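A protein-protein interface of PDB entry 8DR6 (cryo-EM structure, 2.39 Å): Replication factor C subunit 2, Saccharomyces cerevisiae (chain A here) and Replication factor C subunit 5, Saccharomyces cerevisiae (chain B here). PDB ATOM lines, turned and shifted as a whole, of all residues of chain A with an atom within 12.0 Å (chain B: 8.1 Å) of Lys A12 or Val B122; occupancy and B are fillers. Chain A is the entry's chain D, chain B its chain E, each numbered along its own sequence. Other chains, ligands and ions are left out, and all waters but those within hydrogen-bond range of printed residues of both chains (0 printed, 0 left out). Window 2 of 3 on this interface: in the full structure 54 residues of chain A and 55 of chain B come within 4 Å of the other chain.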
ATOM      1  N   ARG A  11      -5.042 -15.217 -13.595  1.00  0.00           N
ATOM      2  CA  ARG A  11      -4.866 -14.099 -14.514  1.00  0.00           C
ATOM      3  C   ARG A  11      -3.726 -14.374 -15.489  1.00  0.00           C
ATOM      4  O   ARG A  11      -3.076 -15.417 -15.420  1.00  0.00           O
ATOM      5  CB  ARG A  11      -4.594 -12.807 -13.739  1.00  0.00           C
ATOM      6  N   LYS A  12      -3.491 -13.430 -16.398  1.00  0.00           N
ATOM      7  CA  LYS A  12      -2.439 -13.559 -17.395  1.00  0.00           C
ATOM      8  C   LYS A  12      -1.842 -12.188 -17.674  1.00  0.00           C
ATOM      9  O   LYS A  12      -2.474 -11.154 -17.444  1.00  0.00           O
ATOM     10  CB  LYS A  12      -2.969 -14.181 -18.695  1.00  0.00           C
ATOM     11  CG  LYS A  12      -1.937 -14.999 -19.454  1.00  0.00           C
ATOM     12  CD  LYS A  12      -1.779 -16.387 -18.858  1.00  0.00           C
ATOM     13  CE  LYS A  12      -0.717 -17.190 -19.592  1.00  0.00           C
ATOM     14  NZ  LYS A  12      -0.561 -18.559 -19.030  1.00  0.00           N
ATOM     15  N   ILE A  13      -0.610 -12.193 -18.175  1.00  0.00           N
ATOM     16  CA  ILE A  13       0.110 -10.973 -18.517  1.00  0.00           C
ATOM     17  C   ILE A  13       0.447 -11.007 -20.001  1.00  0.00           C
ATOM     18  O   ILE A  13       0.845 -12.042 -20.546  1.00  0.00           O
ATOM     19  CB  ILE A  13       1.394 -10.801 -17.677  1.00  0.00           C
ATOM     20  CG1 ILE A  13       1.044 -10.541 -16.211  1.00  0.00           C
ATOM     21  CG2 ILE A  13       2.230  -9.657 -18.230  1.00  0.00           C
ATOM     22  CD1 ILE A  13       2.195 -10.798 -15.257  1.00  0.00           C
ATOM     23  N   SER A  14       0.283  -9.860 -20.655  1.00  0.00           N
ATOM     24  CA  SER A  14       0.609  -9.752 -22.069  1.00  0.00           C
ATOM     25  C   SER A  14       2.093 -10.021 -22.288  1.00  0.00           C
ATOM     26  O   SER A  14       2.940  -9.543 -21.528  1.00  0.00           O
ATOM     27  CB  SER A  14       0.238  -8.366 -22.593  1.00  0.00           C
ATOM     28  OG  SER A  14       0.898  -7.350 -21.857  1.00  0.00           O
ATOM     29  N   LYS A  15       2.405 -10.789 -23.330  1.00  0.00           N
ATOM     30  CA  LYS A  15       3.791 -11.128 -23.619  1.00  0.00           C
ATOM     31  C   LYS A  15       4.577  -9.880 -24.000  1.00  0.00           C
ATOM     32  O   LYS A  15       4.059  -8.961 -24.640  1.00  0.00           O
ATOM     33  CB  LYS A  15       3.860 -12.161 -24.746  1.00  0.00           C
ATOM     34  CG  LYS A  15       3.325 -13.529 -24.359  1.00  0.00           C
ATOM     35  CD  LYS A  15       3.571 -14.556 -25.453  1.00  0.00           C
ATOM     36  CE  LYS A  15       3.053 -15.928 -25.052  1.00  0.00           C
ATOM     37  NZ  LYS A  15       3.220 -16.929 -26.142  1.00  0.00           N
ATOM     38  N   LEU A  16       5.844  -9.854 -23.598  1.00  0.00           N
ATOM     39  CA  LEU A  16       6.721  -8.724 -23.860  1.00  0.00           C
ATOM     40  C   LEU A  16       7.467  -8.911 -25.177  1.00  0.00           C
ATOM     41  O   LEU A  16       7.685 -10.030 -25.646  1.00  0.00           O
ATOM     42  CB  LEU A  16       7.724  -8.545 -22.721  1.00  0.00           C
ATOM     43  CG  LEU A  16       7.321  -7.570 -21.613  1.00  0.00           C
ATOM     44  CD1 LEU A  16       8.160  -7.809 -20.369  1.00  0.00           C
ATOM     45  CD2 LEU A  16       7.452  -6.131 -22.084  1.00  0.00           C
ATOM     46  N   GLN A  24      15.555  -4.740 -20.007  1.00  0.00           N
ATOM     47  CA  GLN A  24      15.472  -4.838 -18.553  1.00  0.00           C
ATOM     48  C   GLN A  24      16.264  -6.024 -18.012  1.00  0.00           C
ATOM     49  O   GLN A  24      16.068  -6.420 -16.858  1.00  0.00           O
ATOM     50  CB  GLN A  24      14.011  -4.932 -18.110  1.00  0.00           C
ATOM     51  CG  GLN A  24      13.396  -6.312 -18.279  1.00  0.00           C
ATOM     52  CD  GLN A  24      11.881  -6.276 -18.313  1.00  0.00           C
ATOM     53  OE1 GLN A  24      11.259  -5.349 -17.794  1.00  0.00           O
ATOM     54  NE2 GLN A  24      11.279  -7.287 -18.926  1.00  0.00           N
ATOM     55  N   MET B 119       9.680 -21.562 -17.149  1.00  0.00           N
ATOM     56  CA  MET B 119       8.303 -21.107 -17.008  1.00  0.00           C
ATOM     57  C   MET B 119       8.316 -19.607 -16.757  1.00  0.00           C
ATOM     58  O   MET B 119       8.955 -19.140 -15.809  1.00  0.00           O
ATOM     59  CB  MET B 119       7.598 -21.834 -15.860  1.00  0.00           C
ATOM     60  CG  MET B 119       6.085 -21.675 -15.859  1.00  0.00           C
ATOM     61  SD  MET B 119       5.371 -21.472 -14.212  1.00  0.00           S
ATOM     62  CE  MET B 119       6.346 -22.621 -13.242  1.00  0.00           C
ATOM     63  N   GLU B 120       7.614 -18.857 -17.602  1.00  0.00           N
ATOM     64  CA  GLU B 120       7.527 -17.417 -17.433  1.00  0.00           C
ATOM     65  C   GLU B 120       6.468 -17.062 -16.392  1.00  0.00           C
ATOM     66  O   GLU B 120       5.589 -17.863 -16.060  1.00  0.00           O
ATOM     67  CB  GLU B 120       7.201 -16.738 -18.763  1.00  0.00           C
ATOM     68  CG  GLU B 120       8.084 -17.187 -19.917  1.00  0.00           C
ATOM     69  CD  GLU B 120       7.946 -16.303 -21.141  1.00  0.00           C
ATOM     70  OE1 GLU B 120       7.313 -15.232 -21.036  1.00  0.00           O
ATOM     71  OE2 GLU B 120       8.470 -16.680 -22.211  1.00  0.00           O
ATOM     72  N   GLN B 121       6.564 -15.840 -15.874  1.00  0.00           N
ATOM     73  CA  GLN B 121       5.634 -15.345 -14.864  1.00  0.00           C
ATOM     74  C   GLN B 121       4.404 -14.785 -15.569  1.00  0.00           C
ATOM     75  O   GLN B 121       4.502 -13.816 -16.330  1.00  0.00           O
ATOM     76  CB  GLN B 121       6.301 -14.285 -13.991  1.00  0.00           C
ATOM     77  CG  GLN B 121       5.327 -13.500 -13.116  1.00  0.00           C
ATOM     78  CD  GLN B 121       6.007 -12.635 -12.060  1.00  0.00           C
ATOM     79  OE1 GLN B 121       5.331 -11.981 -11.265  1.00  0.00           O
ATOM     80  NE2 GLN B 121       7.338 -12.614 -12.051  1.00  0.00           N
ATOM     81  N   VAL B 122       3.247 -15.394 -15.313  1.00  0.00           N
ATOM     82  CA  VAL B 122       2.001 -14.962 -15.922  1.00  0.00           C
ATOM     83  C   VAL B 122       1.057 -14.306 -14.918  1.00  0.00           C
ATOM     84  O   VAL B 122       0.189 -13.524 -15.326  1.00  0.00           O
ATOM     85  CB  VAL B 122       1.305 -16.146 -16.627  1.00  0.00           C
ATOM     86  CG1 VAL B 122       2.262 -16.827 -17.595  1.00  0.00           C
ATOM     87  CG2 VAL B 122       0.773 -17.142 -15.605  1.00  0.00           C
ATOM     88  N   ASP B 123       1.193 -14.598 -13.627  1.00  0.00           N
ATOM     89  CA  ASP B 123       0.337 -13.973 -12.629  1.00  0.00           C
ATOM     90  C   ASP B 123       0.608 -12.475 -12.564  1.00  0.00           C
ATOM     91  O   ASP B 123       1.757 -12.030 -12.626  1.00  0.00           O
ATOM     92  CB  ASP B 123       0.568 -14.611 -11.259  1.00  0.00           C
ATOM     93  CG  ASP B 123       0.263 -16.096 -11.250  1.00  0.00           C
ATOM     94  OD1 ASP B 123      -0.081 -16.640 -12.320  1.00  0.00           O
ATOM     95  OD2 ASP B 123       0.368 -16.720 -10.173  1.00  0.00           O
ATOM     96  N   PHE B 124      -0.463 -11.695 -12.433  1.00  0.00           N
ATOM     97  CA  PHE B 124      -0.367 -10.235 -12.421  1.00  0.00           C
ATOM     98  C   PHE B 124       0.170  -9.795 -11.064  1.00  0.00           C
ATOM     99  O   PHE B 124      -0.585  -9.482 -10.141  1.00  0.00           O
ATOM    100  CB  PHE B 124      -1.722  -9.604 -12.716  1.00  0.00           C
ATOM    101  CG  PHE B 124      -1.676  -8.107 -12.844  1.00  0.00           C
ATOM    102  CD1 PHE B 124      -0.862  -7.504 -13.788  1.00  0.00           C
ATOM    103  CD2 PHE B 124      -2.447  -7.304 -12.020  1.00  0.00           C
ATOM    104  CE1 PHE B 124      -0.817  -6.127 -13.909  1.00  0.00           C
ATOM    105  CE2 PHE B 124      -2.406  -5.927 -12.136  1.00  0.00           C
ATOM    106  CZ  PHE B 124      -1.590  -5.338 -13.082  1.00  0.00           C
ATOM    107  N   GLN B 125       1.496  -9.770 -10.945  1.00  0.00           N
ATOM    108  CA  GLN B 125       2.162  -9.310  -9.725  1.00  0.00           C
ATOM    109  C   GLN B 125       2.580  -7.849  -9.904  1.00  0.00           C
ATOM    110  O   GLN B 125       3.743  -7.519 -10.145  1.00  0.00           O
ATOM    111  CB  GLN B 125       3.354 -10.200  -9.401  1.00  0.00           C
ATOM    112  CG  GLN B 125       2.994 -11.656  -9.155  1.00  0.00           C
ATOM    113  CD  GLN B 125       4.135 -12.438  -8.533  1.00  0.00           C
ATOM    114  OE1 GLN B 125       5.292 -12.022  -8.589  1.00  0.00           O
ATOM    115  NE2 GLN B 125       3.812 -13.579  -7.935  1.00  0.00           N
ATOM    116  N   ALA B 132       3.659  -5.420 -13.956  1.00  0.00           N
ATOM    117  CA  ALA B 132       3.794  -6.655 -13.199  1.00  0.00           C
ATOM    118  C   ALA B 132       5.241  -7.139 -13.186  1.00  0.00           C
ATOM    119  O   ALA B 132       6.027  -6.852 -14.093  1.00  0.00           O
ATOM    120  CB  ALA B 132       2.891  -7.739 -13.786  1.00  0.00           C
ATOM    121  N   HIS B 133       5.587  -7.882 -12.138  1.00  0.00           N
ATOM    122  CA  HIS B 133       6.904  -8.490 -12.047  1.00  0.00           C
ATOM    123  C   HIS B 133       7.068  -9.559 -13.125  1.00  0.00           C
ATOM    124  O   HIS B 133       6.096 -10.138 -13.619  1.00  0.00           O
ATOM    125  CB  HIS B 133       7.121  -9.103 -10.663  1.00  0.00           C
ATOM    126  CG  HIS B 133       7.047  -8.112  -9.544  1.00  0.00           C
ATOM    127  ND1 HIS B 133       6.034  -8.118  -8.610  1.00  0.00           N
ATOM    128  CD2 HIS B 133       7.864  -7.085  -9.207  1.00  0.00           C
ATOM    129  CE1 HIS B 133       6.228  -7.136  -7.748  1.00  0.00           C
ATOM    130  NE2 HIS B 133       7.331  -6.495  -8.087  1.00  0.00           N
ATOM    131  N   ARG B 134       8.325  -9.816 -13.490  1.00  0.00           N
ATOM    132  CA  ARG B 134       8.639 -10.715 -14.590  1.00  0.00           C
ATOM    133  C   ARG B 134       9.540 -11.880 -14.208  1.00  0.00           C
ATOM    134  O   ARG B 134       9.745 -12.771 -15.040  1.00  0.00           O
ATOM    135  CB  ARG B 134       9.300  -9.933 -15.736  1.00  0.00           C
ATOM    136  CG  ARG B 134       8.320  -9.485 -16.807  1.00  0.00           C
ATOM    137  CD  ARG B 134       7.523  -8.271 -16.344  1.00  0.00           C
ATOM    138  NE  ARG B 134       6.818  -7.607 -17.433  1.00  0.00           N
ATOM    139  CZ  ARG B 134       5.841  -8.155 -18.144  1.00  0.00           C
ATOM    140  NH1 ARG B 134       5.412  -9.383 -17.902  1.00  0.00           N
ATOM    141  NH2 ARG B 134       5.276  -7.450 -19.120  1.00  0.00           N
ATOM    142  N   TYR B 135      10.083 -11.907 -12.993  1.00  0.00           N
ATOM    143  CA  TYR B 135      10.967 -12.980 -12.562  1.00  0.00           C
ATOM    144  C   TYR B 135      10.626 -13.413 -11.142  1.00  0.00           C
ATOM    145  O   TYR B 135      10.088 -12.635 -10.347  1.00  0.00           O
ATOM    146  CB  TYR B 135      12.441 -12.549 -12.639  1.00  0.00           C
ATOM    147  CG  TYR B 135      12.808 -11.385 -11.744  1.00  0.00           C
ATOM    148  CD1 TYR B 135      13.013 -11.563 -10.382  1.00  0.00           C
ATOM    149  CD2 TYR B 135      12.955 -10.106 -12.264  1.00  0.00           C
ATOM    150  CE1 TYR B 135      13.350 -10.503  -9.564  1.00  0.00           C
ATOM    151  CE2 TYR B 135      13.291  -9.039 -11.453  1.00  0.00           C
ATOM    152  CZ  TYR B 135      13.487  -9.243 -10.105  1.00  0.00           C
ATOM    153  OH  TYR B 135      13.822  -8.183  -9.294  1.00  0.00           O
ATOM    154  N   LYS B 136      10.946 -14.666 -10.836  1.00  0.00           N
ATOM    155  CA  LYS B 136      10.782 -15.228  -9.504  1.00  0.00           C
ATOM    156  C   LYS B 136      12.147 -15.503  -8.887  1.00  0.00           C
ATOM    157  O   LYS B 136      13.059 -16.006  -9.550  1.00  0.00           O
ATOM    158  CB  LYS B 136       9.962 -16.520  -9.552  1.00  0.00           C
ATOM    159  CG  LYS B 136       8.527 -16.360  -9.074  1.00  0.00           C
ATOM    160  CD  LYS B 136       7.752 -17.666  -9.177  1.00  0.00           C
ATOM    161  CE  LYS B 136       8.130 -18.638  -8.069  1.00  0.00           C
ATOM    162  NZ  LYS B 136       7.570 -18.233  -6.750  1.00  0.00           N
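Printed residues of chain B that touch a printed residue of chain A: Gln B121, Val B122, Asp B123, Phe B124, Ala B132 and Arg B134.
The backbone NH (N) of Ile A13 sits close to the backbone carbonyl oxygen (O) of Val B122 (3.2 Å).
Among the printed residues, pairs that only touch across the chains: Arg A11 with Val B122, Lys A12 with Val B122, Ile A13 with Gln B121, Ile A13 with Asp B123, Ile A13 with Phe B124, Ile A13 with Ala B132, Ile A13 with Arg B134, Ser A14 with Arg B134 and Leu A16 with Arg B134.
Of chain B, only Val B122 (3.8 Å) comes within 4 Å of Arg A11.
Lys A12 touches one residue of chain B.
Of the printed residues of chain B, Ile A13 touches Gln B121 (3.9 Å), Val B122 (3.2 Å), Asp B123 (2.9 Å), Phe B124 (3.9 Å), Ala B132 (3.5 Å) and Arg B134 (3.2 Å).
Printed residues of chain B within 4 Å of Ser A14: Arg B134.
No residue of chain A comes within 4 Å of Glu B120.
Gln B121 touches just one residue of chain A: Ile A13.
Of the printed residues of chain A, Asp B123 touches Ile A13 (2.9 Å).
Phe B124 touches one residue of chain A.
Printed residues of chain A within 4 Å of Ala B132: Ile A13.
Printed residues of chain A within 4 Å of Arg B134: Ile A13 (3.2 Å), Ser A14 (3.95 Å) and Leu A16 (3.2 Å).
The nearest residue of chain A that does not touch Val B122 is Ser A14 (6.5 Å).
The nearest printed residue of chain A that does not touch Arg B134 is Gln A24 (4.3 Å).
The side-chain amide nitrogen of Gln B121 lies close to the backbone NH of Tyr B135, at 3.0 Å.
O of His B133 lies close to OE1 of Gln B121.
The side-chain amide nitrogen (NE2) of Gln B121 lies close to the backbone NH (N) of Arg B134 (3.3 Å).
The side-chain amide oxygen of Gln B121 lies close to the side-chain amide oxygen of Gln B125 (2.7 Å).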
